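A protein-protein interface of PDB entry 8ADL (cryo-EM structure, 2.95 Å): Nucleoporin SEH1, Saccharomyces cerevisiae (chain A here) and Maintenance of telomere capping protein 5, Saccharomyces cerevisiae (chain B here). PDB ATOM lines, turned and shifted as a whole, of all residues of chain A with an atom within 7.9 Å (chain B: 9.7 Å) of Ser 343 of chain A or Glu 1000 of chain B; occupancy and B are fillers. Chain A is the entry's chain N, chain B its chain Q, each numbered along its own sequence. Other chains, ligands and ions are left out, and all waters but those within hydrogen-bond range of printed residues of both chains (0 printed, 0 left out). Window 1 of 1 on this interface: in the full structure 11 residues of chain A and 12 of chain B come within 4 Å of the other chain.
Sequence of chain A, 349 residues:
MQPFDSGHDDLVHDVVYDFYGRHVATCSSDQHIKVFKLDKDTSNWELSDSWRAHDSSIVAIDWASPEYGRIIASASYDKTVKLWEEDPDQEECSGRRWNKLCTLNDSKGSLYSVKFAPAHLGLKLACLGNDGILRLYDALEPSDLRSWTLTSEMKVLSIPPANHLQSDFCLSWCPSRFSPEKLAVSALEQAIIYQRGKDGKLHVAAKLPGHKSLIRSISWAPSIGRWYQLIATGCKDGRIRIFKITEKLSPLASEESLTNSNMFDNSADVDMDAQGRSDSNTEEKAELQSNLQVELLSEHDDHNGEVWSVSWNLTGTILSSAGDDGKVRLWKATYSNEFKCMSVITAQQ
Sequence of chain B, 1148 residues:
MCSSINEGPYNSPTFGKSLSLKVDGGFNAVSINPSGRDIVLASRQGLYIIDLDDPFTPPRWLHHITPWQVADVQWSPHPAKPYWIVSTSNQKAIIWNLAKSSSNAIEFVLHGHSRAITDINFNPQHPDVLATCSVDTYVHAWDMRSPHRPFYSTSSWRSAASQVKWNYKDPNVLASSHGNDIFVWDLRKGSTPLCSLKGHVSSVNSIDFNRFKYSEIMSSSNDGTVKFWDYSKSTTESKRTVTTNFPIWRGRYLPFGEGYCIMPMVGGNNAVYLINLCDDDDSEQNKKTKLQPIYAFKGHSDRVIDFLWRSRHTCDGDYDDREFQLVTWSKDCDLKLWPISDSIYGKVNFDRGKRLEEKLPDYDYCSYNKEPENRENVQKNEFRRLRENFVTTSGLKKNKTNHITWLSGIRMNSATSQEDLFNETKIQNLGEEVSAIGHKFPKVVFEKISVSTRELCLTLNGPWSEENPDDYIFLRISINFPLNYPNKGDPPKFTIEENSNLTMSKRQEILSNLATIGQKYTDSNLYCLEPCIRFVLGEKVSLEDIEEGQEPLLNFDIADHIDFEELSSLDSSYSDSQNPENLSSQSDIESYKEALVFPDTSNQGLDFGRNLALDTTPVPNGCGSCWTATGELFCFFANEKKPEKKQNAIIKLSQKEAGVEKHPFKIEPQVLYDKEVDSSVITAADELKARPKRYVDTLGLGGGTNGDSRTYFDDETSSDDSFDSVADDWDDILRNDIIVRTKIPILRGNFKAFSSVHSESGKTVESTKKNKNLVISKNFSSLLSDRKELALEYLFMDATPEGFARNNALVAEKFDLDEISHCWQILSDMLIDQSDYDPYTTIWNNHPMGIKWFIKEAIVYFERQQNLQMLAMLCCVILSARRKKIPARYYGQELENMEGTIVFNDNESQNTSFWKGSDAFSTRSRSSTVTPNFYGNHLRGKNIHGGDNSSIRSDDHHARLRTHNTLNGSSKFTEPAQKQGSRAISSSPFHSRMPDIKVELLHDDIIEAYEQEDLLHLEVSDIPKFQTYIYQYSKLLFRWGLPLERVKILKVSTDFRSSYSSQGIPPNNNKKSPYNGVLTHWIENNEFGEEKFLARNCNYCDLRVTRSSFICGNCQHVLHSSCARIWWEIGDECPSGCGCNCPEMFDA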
ATOM      1  N   HIS A 303     -13.400 -17.843  18.658  1.00  0.00           N
ATOM      2  CA  HIS A 303     -13.869 -17.180  17.448  1.00  0.00           C
ATOM      3  C   HIS A 303     -14.030 -18.232  16.359  1.00  0.00           C
ATOM      4  O   HIS A 303     -13.040 -18.726  15.811  1.00  0.00           O
ATOM      5  CB  HIS A 303     -12.887 -16.098  17.008  1.00  0.00           C
ATOM      6  CG  HIS A 303     -12.938 -14.853  17.836  1.00  0.00           C
ATOM      7  ND1 HIS A 303     -13.910 -13.889  17.673  1.00  0.00           N
ATOM      8  CD2 HIS A 303     -12.133 -14.410  18.829  1.00  0.00           C
ATOM      9  CE1 HIS A 303     -13.703 -12.908  18.533  1.00  0.00           C
ATOM     10  NE2 HIS A 303     -12.631 -13.200  19.247  1.00  0.00           N
ATOM     11  N   ILE A 318      -6.792  -7.325  30.574  1.00  0.00           N
ATOM     12  CA  ILE A 318      -7.910  -7.617  29.686  1.00  0.00           C
ATOM     13  C   ILE A 318      -7.422  -7.521  28.248  1.00  0.00           C
ATOM     14  O   ILE A 318      -6.734  -6.561  27.880  1.00  0.00           O
ATOM     15  CB  ILE A 318      -9.089  -6.663  29.934  1.00  0.00           C
ATOM     16  CG1 ILE A 318      -9.282  -6.439  31.433  1.00  0.00           C
ATOM     17  CG2 ILE A 318     -10.357  -7.229  29.327  1.00  0.00           C
ATOM     18  CD1 ILE A 318     -10.381  -5.455  31.764  1.00  0.00           C
ATOM     19  N   LEU A 319      -7.779  -8.512  27.438  1.00  0.00           N
ATOM     20  CA  LEU A 319      -7.359  -8.587  26.047  1.00  0.00           C
ATOM     21  C   LEU A 319      -8.581  -8.606  25.144  1.00  0.00           C
ATOM     22  O   LEU A 319      -9.497  -9.407  25.353  1.00  0.00           O
ATOM     23  CB  LEU A 319      -6.508  -9.835  25.802  1.00  0.00           C
ATOM     24  CG  LEU A 319      -6.315 -10.247  24.344  1.00  0.00           C
ATOM     25  CD1 LEU A 319      -5.373  -9.286  23.653  1.00  0.00           C
ATOM     26  CD2 LEU A 319      -5.795 -11.667  24.252  1.00  0.00           C
ATOM     27  N   SER A 321     -10.277  -9.099  21.256  1.00  0.00           N
ATOM     28  CA  SER A 321     -10.066  -9.958  20.096  1.00  0.00           C
ATOM     29  C   SER A 321     -11.257  -9.793  19.170  1.00  0.00           C
ATOM     30  O   SER A 321     -12.381 -10.147  19.540  1.00  0.00           O
ATOM     31  CB  SER A 321      -9.904 -11.415  20.516  1.00  0.00           C
ATOM     32  OG  SER A 321     -11.080 -11.902  21.137  1.00  0.00           O
ATOM     33  N   LYS A 327     -17.850 -10.013  15.810  1.00  0.00           N
ATOM     34  CA  LYS A 327     -17.887 -10.227  17.248  1.00  0.00           C
ATOM     35  C   LYS A 327     -16.561  -9.809  17.867  1.00  0.00           C
ATOM     36  O   LYS A 327     -15.495 -10.022  17.280  1.00  0.00           O
ATOM     37  CB  LYS A 327     -18.187 -11.693  17.575  1.00  0.00           C
ATOM     38  CG  LYS A 327     -19.642 -12.084  17.367  1.00  0.00           C
ATOM     39  CD  LYS A 327     -19.984 -13.371  18.099  1.00  0.00           C
ATOM     40  CE  LYS A 327     -21.447 -13.743  17.910  1.00  0.00           C
ATOM     41  NZ  LYS A 327     -21.737 -14.176  16.516  1.00  0.00           N
ATOM     42  N   VAL A 328     -16.634  -9.208  19.051  1.00  0.00           N
ATOM     43  CA  VAL A 328     -15.462  -8.775  19.802  1.00  0.00           C
ATOM     44  C   VAL A 328     -15.533  -9.403  21.185  1.00  0.00           C
ATOM     45  O   VAL A 328     -16.537  -9.247  21.889  1.00  0.00           O
ATOM     46  CB  VAL A 328     -15.386  -7.241  19.893  1.00  0.00           C
ATOM     47  CG1 VAL A 328     -14.390  -6.807  20.958  1.00  0.00           C
ATOM     48  CG2 VAL A 328     -15.016  -6.658  18.543  1.00  0.00           C
ATOM     49  N   ARG A 329     -14.476 -10.114  21.571  1.00  0.00           N
ATOM     50  CA  ARG A 329     -14.440 -10.823  22.841  1.00  0.00           C
ATOM     51  C   ARG A 329     -13.352 -10.250  23.738  1.00  0.00           C
ATOM     52  O   ARG A 329     -12.267  -9.890  23.268  1.00  0.00           O
ATOM     53  CB  ARG A 329     -14.212 -12.322  22.632  1.00  0.00           C
ATOM     54  CG  ARG A 329     -15.461 -13.082  22.216  1.00  0.00           C
ATOM     55  CD  ARG A 329     -15.142 -14.520  21.848  1.00  0.00           C
ATOM     56  NE  ARG A 329     -16.349 -15.291  21.575  1.00  0.00           N
ATOM     57  CZ  ARG A 329     -16.801 -15.576  20.362  1.00  0.00           C
ATOM     58  NH1 ARG A 329     -16.170 -15.164  19.274  1.00  0.00           N
ATOM     59  NH2 ARG A 329     -17.914 -16.292  20.236  1.00  0.00           N
ATOM     60  N   LEU A 330     -13.654 -10.171  25.031  1.00  0.00           N
ATOM     61  CA  LEU A 330     -12.736  -9.671  26.046  1.00  0.00           C
ATOM     62  C   LEU A 330     -12.278 -10.825  26.926  1.00  0.00           C
ATOM     63  O   LEU A 330     -13.107 -11.581  27.442  1.00  0.00           O
ATOM     64  CB  LEU A 330     -13.398  -8.587  26.899  1.00  0.00           C
ATOM     65  CG  LEU A 330     -14.088  -7.438  26.164  1.00  0.00           C
ATOM     66  CD1 LEU A 330     -14.559  -6.382  27.149  1.00  0.00           C
ATOM     67  CD2 LEU A 330     -13.166  -6.827  25.126  1.00  0.00           C
ATOM     68  N   TRP A 331     -10.966 -10.959  27.101  1.00  0.00           N
ATOM     69  CA  TRP A 331     -10.388 -12.069  27.845  1.00  0.00           C
ATOM     70  C   TRP A 331      -9.676 -11.538  29.078  1.00  0.00           C
ATOM     71  O   TRP A 331      -8.800 -10.675  28.967  1.00  0.00           O
ATOM     72  CB  TRP A 331      -9.405 -12.872  26.990  1.00  0.00           C
ATOM     73  CG  TRP A 331      -9.903 -13.201  25.623  1.00  0.00           C
ATOM     74  CD1 TRP A 331      -9.896 -12.390  24.526  1.00  0.00           C
ATOM     75  CD2 TRP A 331     -10.511 -14.427  25.210  1.00  0.00           C
ATOM     76  NE1 TRP A 331     -10.447 -13.042  23.451  1.00  0.00           N
ATOM     77  CE2 TRP A 331     -10.834 -14.294  23.847  1.00  0.00           C
ATOM     78  CE3 TRP A 331     -10.808 -15.628  25.859  1.00  0.00           C
ATOM     79  CZ2 TRP A 331     -11.438 -15.313  23.122  1.00  0.00           C
ATOM     80  CZ3 TRP A 331     -11.407 -16.637  25.141  1.00  0.00           C
ATOM     81  CH2 TRP A 331     -11.715 -16.474  23.786  1.00  0.00           C
ATOM     82  N   LYS A 332     -10.036 -12.069  30.242  1.00  0.00           N
ATOM     83  CA  LYS A 332      -9.390 -11.734  31.501  1.00  0.00           C
ATOM     84  C   LYS A 332      -8.921 -13.017  32.169  1.00  0.00           C
ATOM     85  O   LYS A 332      -9.620 -14.034  32.134  1.00  0.00           O
ATOM     86  CB  LYS A 332     -10.340 -10.966  32.434  1.00  0.00           C
ATOM     87  CG  LYS A 332      -9.704 -10.501  33.739  1.00  0.00           C
ATOM     88  CD  LYS A 332     -10.711  -9.806  34.637  1.00  0.00           C
ATOM     89  CE  LYS A 332     -10.862  -8.340  34.272  1.00  0.00           C
ATOM     90  NZ  LYS A 332      -9.646  -7.558  34.633  1.00  0.00           N
ATOM     91  N   LYS A 340     -10.071 -16.561  30.369  1.00  0.00           N
ATOM     92  CA  LYS A 340     -11.410 -16.966  29.973  1.00  0.00           C
ATOM     93  C   LYS A 340     -12.147 -15.763  29.409  1.00  0.00           C
ATOM     94  O   LYS A 340     -11.841 -14.616  29.745  1.00  0.00           O
ATOM     95  CB  LYS A 340     -12.206 -17.566  31.138  1.00  0.00           C
ATOM     96  CG  LYS A 340     -11.919 -19.035  31.395  1.00  0.00           C
ATOM     97  CD  LYS A 340     -12.810 -19.587  32.495  1.00  0.00           C
ATOM     98  CE  LYS A 340     -14.260 -19.660  32.041  1.00  0.00           C
ATOM     99  NZ  LYS A 340     -15.143 -20.252  33.083  1.00  0.00           N
ATOM    100  N   CYS A 341     -13.117 -16.037  28.540  1.00  0.00           N
ATOM    101  CA  CYS A 341     -13.873 -14.971  27.898  1.00  0.00           C
ATOM    102  C   CYS A 341     -14.788 -14.294  28.909  1.00  0.00           C
ATOM    103  O   CYS A 341     -15.526 -14.961  29.640  1.00  0.00           O
ATOM    104  CB  CYS A 341     -14.686 -15.526  26.733  1.00  0.00           C
ATOM    105  SG  CYS A 341     -15.406 -14.260  25.669  1.00  0.00           S
ATOM    106  N   MET A 342     -14.744 -12.965  28.944  1.00  0.00           N
ATOM    107  CA  MET A 342     -15.558 -12.188  29.867  1.00  0.00           C
ATOM    108  C   MET A 342     -16.823 -11.641  29.220  1.00  0.00           C
ATOM    109  O   MET A 342     -17.892 -11.670  29.839  1.00  0.00           O
ATOM    110  CB  MET A 342     -14.722 -11.040  30.454  1.00  0.00           C
ATOM    111  CG  MET A 342     -15.511  -9.854  30.989  1.00  0.00           C
ATOM    112  SD  MET A 342     -14.456  -8.484  31.493  1.00  0.00           S
ATOM    113  CE  MET A 342     -14.529  -8.641  33.274  1.00  0.00           C
ATOM    114  N   SER A 343     -16.743 -11.182  27.972  1.00  0.00           N
ATOM    115  CA  SER A 343     -17.923 -10.681  27.286  1.00  0.00           C
ATOM    116  C   SER A 343     -17.773 -10.875  25.787  1.00  0.00           C
ATOM    117  O   SER A 343     -16.668 -11.025  25.262  1.00  0.00           O
ATOM    118  CB  SER A 343     -18.180  -9.207  27.605  1.00  0.00           C
ATOM    119  OG  SER A 343     -18.519  -9.048  28.968  1.00  0.00           O
ATOM    120  N   VAL A 344     -18.916 -10.875  25.108  1.00  0.00           N
ATOM    121  CA  VAL A 344     -19.003 -10.917  23.654  1.00  0.00           C
ATOM    122  C   VAL A 344     -19.780  -9.690  23.200  1.00  0.00           C
ATOM    123  O   VAL A 344     -20.884  -9.434  23.694  1.00  0.00           O
ATOM    124  CB  VAL A 344     -19.677 -12.210  23.156  1.00  0.00           C
ATOM    125  CG1 VAL A 344     -19.715 -12.236  21.639  1.00  0.00           C
ATOM    126  CG2 VAL A 344     -18.948 -13.435  23.689  1.00  0.00           C
ATOM    127  N   ILE A 345     -19.209  -8.934  22.266  1.00  0.00           N
ATOM    128  CA  ILE A 345     -19.837  -7.726  21.745  1.00  0.00           C
ATOM    129  C   ILE A 345     -20.294  -8.008  20.322  1.00  0.00           C
ATOM    130  O   ILE A 345     -19.476  -8.312  19.446  1.00  0.00           O
ATOM    131  CB  ILE A 345     -18.875  -6.530  21.780  1.00  0.00           C
ATOM    132  CG1 ILE A 345     -18.283  -6.352  23.180  1.00  0.00           C
ATOM    133  CG2 ILE A 345     -19.588  -5.270  21.327  1.00  0.00           C
ATOM    134  CD1 ILE A 345     -19.310  -6.081  24.247  1.00  0.00           C
ATOM    135  N   THR A 346     -21.600  -7.901  20.095  1.00  0.00           N
ATOM    136  CA  THR A 346     -22.212  -8.161  18.799  1.00  0.00           C
ATOM    137  C   THR A 346     -22.719  -6.853  18.206  1.00  0.00           C
ATOM    138  O   THR A 346     -23.222  -5.988  18.929  1.00  0.00           O
ATOM    139  CB  THR A 346     -23.363  -9.165  18.940  1.00  0.00           C
ATOM    140  OG1 THR A 346     -22.945 -10.253  19.774  1.00  0.00           O
ATOM    141  CG2 THR A 346     -23.771  -9.726  17.582  1.00  0.00           C
ATOM    142  N   ILE B 997     -25.913  -2.417  19.365  1.00  0.00           N
ATOM    143  CA  ILE B 997     -24.822  -3.206  19.927  1.00  0.00           C
ATOM    144  C   ILE B 997     -25.387  -4.102  21.019  1.00  0.00           C
ATOM    145  O   ILE B 997     -26.032  -3.617  21.958  1.00  0.00           O
ATOM    146  CB  ILE B 997     -23.699  -2.307  20.474  1.00  0.00           C
ATOM    147  CG1 ILE B 997     -23.015  -1.530  19.342  1.00  0.00           C
ATOM    148  CG2 ILE B 997     -22.678  -3.129  21.244  1.00  0.00           C
ATOM    149  CD1 ILE B 997     -23.579  -0.146  19.090  1.00  0.00           C
ATOM    150  N   LYS B 998     -25.149  -5.403  20.901  1.00  0.00           N
ATOM    151  CA  LYS B 998     -25.583  -6.368  21.901  1.00  0.00           C
ATOM    152  C   LYS B 998     -24.391  -6.820  22.734  1.00  0.00           C
ATOM    153  O   LYS B 998     -23.371  -7.252  22.187  1.00  0.00           O
ATOM    154  CB  LYS B 998     -26.257  -7.570  21.238  1.00  0.00           C
ATOM    155  CG  LYS B 998     -26.771  -8.612  22.214  1.00  0.00           C
ATOM    156  CD  LYS B 998     -27.055  -9.927  21.511  1.00  0.00           C
ATOM    157  CE  LYS B 998     -27.591 -10.965  22.482  1.00  0.00           C
ATOM    158  NZ  LYS B 998     -27.759 -12.295  21.837  1.00  0.00           N
ATOM    159  N   VAL B 999     -24.525  -6.719  24.054  1.00  0.00           N
ATOM    160  CA  VAL B 999     -23.459  -7.027  24.999  1.00  0.00           C
ATOM    161  C   VAL B 999     -23.908  -8.211  25.844  1.00  0.00           C
ATOM    162  O   VAL B 999     -24.992  -8.178  26.438  1.00  0.00           O
ATOM    163  CB  VAL B 999     -23.121  -5.816  25.887  1.00  0.00           C
ATOM    164  CG1 VAL B 999     -22.048  -6.176  26.905  1.00  0.00           C
ATOM    165  CG2 VAL B 999     -22.687  -4.633  25.033  1.00  0.00           C
ATOM    166  N   GLU B1000     -23.076  -9.249  25.902  1.00  0.00           N
ATOM    167  CA  GLU B1000     -23.387 -10.470  26.646  1.00  0.00           C
ATOM    168  C   GLU B1000     -22.262 -10.754  27.637  1.00  0.00           C
ATOM    169  O   GLU B1000     -21.192 -11.227  27.248  1.00  0.00           O
ATOM    170  CB  GLU B1000     -23.588 -11.650  25.701  1.00  0.00           C
ATOM    171  CG  GLU B1000     -24.992 -11.775  25.138  1.00  0.00           C
ATOM    172  CD  GLU B1000     -25.119 -12.926  24.160  1.00  0.00           C
ATOM    173  OE1 GLU B1000     -24.129 -13.224  23.460  1.00  0.00           O
ATOM    174  OE2 GLU B1000     -26.208 -13.536  24.093  1.00  0.00           O
ATOM    175  N   LEU B1001     -22.510 -10.466  28.914  1.00  0.00           N
ATOM    176  CA  LEU B1001     -21.550 -10.797  29.960  1.00  0.00           C
ATOM    177  C   LEU B1001     -21.483 -12.308  30.151  1.00  0.00           C
ATOM    178  O   LEU B1001     -22.514 -12.973  30.287  1.00  0.00           O
ATOM    179  CB  LEU B1001     -21.938 -10.121  31.273  1.00  0.00           C
ATOM    180  CG  LEU B1001     -21.508  -8.673  31.507  1.00  0.00           C
ATOM    181  CD1 LEU B1001     -22.335  -8.052  32.618  1.00  0.00           C
ATOM    182  CD2 LEU B1001     -20.035  -8.610  31.856  1.00  0.00           C
ATOM    183  N   LEU B1002     -20.267 -12.845  30.170  1.00  0.00           N
ATOM    184  CA  LEU B1002     -20.025 -14.268  30.389  1.00  0.00           C
ATOM    185  C   LEU B1002     -19.140 -14.417  31.618  1.00  0.00           C
ATOM    186  O   LEU B1002     -17.983 -13.982  31.605  1.00  0.00           O
ATOM    187  CB  LEU B1002     -19.380 -14.914  29.164  1.00  0.00           C
ATOM    188  CG  LEU B1002     -20.147 -14.823  27.845  1.00  0.00           C
ATOM    189  CD1 LEU B1002     -19.474 -15.674  26.782  1.00  0.00           C
ATOM    190  CD2 LEU B1002     -21.593 -15.247  28.028  1.00  0.00           C
ATOM    191  N   HIS B1003     -19.693 -15.032  32.670  1.00  0.00           N
ATOM    192  CA  HIS B1003     -19.003 -15.308  33.934  1.00  0.00           C
ATOM    193  C   HIS B1003     -18.472 -14.023  34.573  1.00  0.00           C
ATOM    194  O   HIS B1003     -17.281 -13.878  34.856  1.00  0.00           O
ATOM    195  CB  HIS B1003     -17.880 -16.337  33.745  1.00  0.00           C
ATOM    196  CG  HIS B1003     -18.325 -17.601  33.079  1.00  0.00           C
ATOM    197  ND1 HIS B1003     -18.164 -17.828  31.730  1.00  0.00           N
ATOM    198  CD2 HIS B1003     -18.926 -18.707  33.578  1.00  0.00           C
ATOM    199  CE1 HIS B1003     -18.646 -19.020  31.425  1.00  0.00           C
ATOM    200  NE2 HIS B1003     -19.114 -19.574  32.529  1.00  0.00           N
ATOM    201  N   ASP B1004     -19.387 -13.082  34.789  1.00  0.00           N
ATOM    202  CA  ASP B1004     -19.035 -11.838  35.459  1.00  0.00           C
ATOM    203  C   ASP B1004     -18.780 -12.089  36.940  1.00  0.00           C
ATOM    204  O   ASP B1004     -19.534 -12.804  37.605  1.00  0.00           O
ATOM    205  CB  ASP B1004     -20.146 -10.805  35.279  1.00  0.00           C
ATOM    206  CG  ASP B1004     -19.717  -9.410  35.687  1.00  0.00           C
ATOM    207  OD1 ASP B1004     -18.694  -8.923  35.161  1.00  0.00           O
ATOM    208  OD2 ASP B1004     -20.404  -8.799  36.533  1.00  0.00           O
ATOM    209  N   ASP B1005     -17.700 -11.496  37.453  1.00  0.00           N
ATOM    210  CA  ASP B1005     -17.318 -11.713  38.846  1.00  0.00           C
ATOM    211  C   ASP B1005     -18.273 -11.028  39.815  1.00  0.00           C
ATOM    212  O   ASP B1005     -18.493 -11.531  40.923  1.00  0.00           O
ATOM    213  CB  ASP B1005     -15.888 -11.226  39.077  1.00  0.00           C
ATOM    214  CG  ASP B1005     -14.851 -12.172  38.505  1.00  0.00           C
ATOM    215  OD1 ASP B1005     -15.145 -13.380  38.395  1.00  0.00           O
ATOM    216  OD2 ASP B1005     -13.743 -11.707  38.166  1.00  0.00           O
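Glu 1000 of chain B touches two residues of chain A.
No residue of chain B comes within 4 Å of Leu 330 of chain A.
Of the printed residues of chain B, Val 344 of chain A touches Lys 998 (3.6 Å), Val 999 (3.8 Å), Glu 1000 (3.1 Å) and Leu 1002 (3.9 Å).
Of the printed residues of chain B, Met 342 of chain A touches Leu 1001 (3.7 Å) and Leu 1002 (2.7 Å).
Of the printed residues of chain B, Ile 345 of chain A touches Ile 997, Lys 998 and Val 999.
Of the printed residues of chain A, Val 999 of chain B touches Val 344 (3.8 Å) and Ile 345 (3.8 Å).
Of the printed residues of chain A, Leu 1002 of chain B touches Cys 341, Met 342 and Val 344.
The nearest printed residue of chain B that does not touch Thr 346 of chain A is Glu 1000 of chain B (4.9 Å).
Met 342 of chain A touches Leu 1001 of chain B.
Ser 343 of chain A touches Glu 1000 of chain B (CA to O, 3.3 Å).
Ser 343 of chain A touches Leu 1001 of chain B.
Val 344 of chain A touches Lys 998 of chain B.
CA of Val 999 of chain B touches O of Val 344 of chain A, 3.8 Å away.
Val 344 of chain A touches Leu 1002 of chain B.
Ile 997 of chain B touches Ile 345 of chain A (CG2 to CG2, 3.8 Å).
Ile 345 of chain A touches Lys 998 of chain B.
Val 999 of chain B touches Ile 345 of chain A (CG2 to CD1, 3.8 Å).
Thr 346 of chain A touches Ile 997 of chain B.
The backbone NH of Thr 346 of chain A is in hydrogen-bond range of the backbone carbonyl oxygen of Lys 998 of chain B (2.8 Å).
The backbone NH (N) of Glu 1000 of chain B is in hydrogen-bond range of the backbone carbonyl oxygen (O) of Val 344 of chain A (3.1 Å).
The backbone carbonyl oxygen (O) of Met 342 of chain A sits at hydrogen-bond distance from the backbone NH (N) of Leu 1002 of chain B, 2.7 Å away.
O of Cys 341 of chain A sits close to O of Leu 1002 of chain B, 3.3 Å away.
O of Val 328 of chain A sits at hydrogen-bond distance from N of Ile 345 of chain A (2.7 Å).
NZ of Lys 998 of chain B lies within salt-bridge range of OE2 of Glu 1000 of chain B (3.0 Å).
The backbone NH of Leu 330 of chain A is in hydrogen-bond range of the backbone carbonyl oxygen of Ser 343 of chain A, 3.1 Å away.
The backbone carbonyl oxygen (O) of Leu 330 of chain A lies within hydrogen-bond range of the backbone NH (N) of Met 342 of chain A (2.6 Å).
O of Ser 343 of chain A lies within hydrogen-bond range of SG of Cys 341 of chain A (3.5 Å).
Of the 9 printed residues of chain B, 6 touch a printed residue of chain A.
Printed residues of chain B that touch a printed residue of chain A: Ile 997, Lys 998, Val 999, Glu 1000, Leu 1001 and Leu 1002.
Hydrophobic or aromatic side chains of chain B that line the printed part of chain A: Ile 997, Val 999, Leu 1001 and Leu 1002.
Hydrophobic or aromatic side chains of chain A that line the printed part of chain B: Val 344 and Ile 345.
Along chain A the printed residues that touch a printed residue of chain B span positions 341 to 346.
Among the printed residues, 14 pairs touch across the chains.
Among the printed residues, no Asp or Glu carboxylate lies within 4 Å of a Lys or Arg side-chain nitrogen of the other chain.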
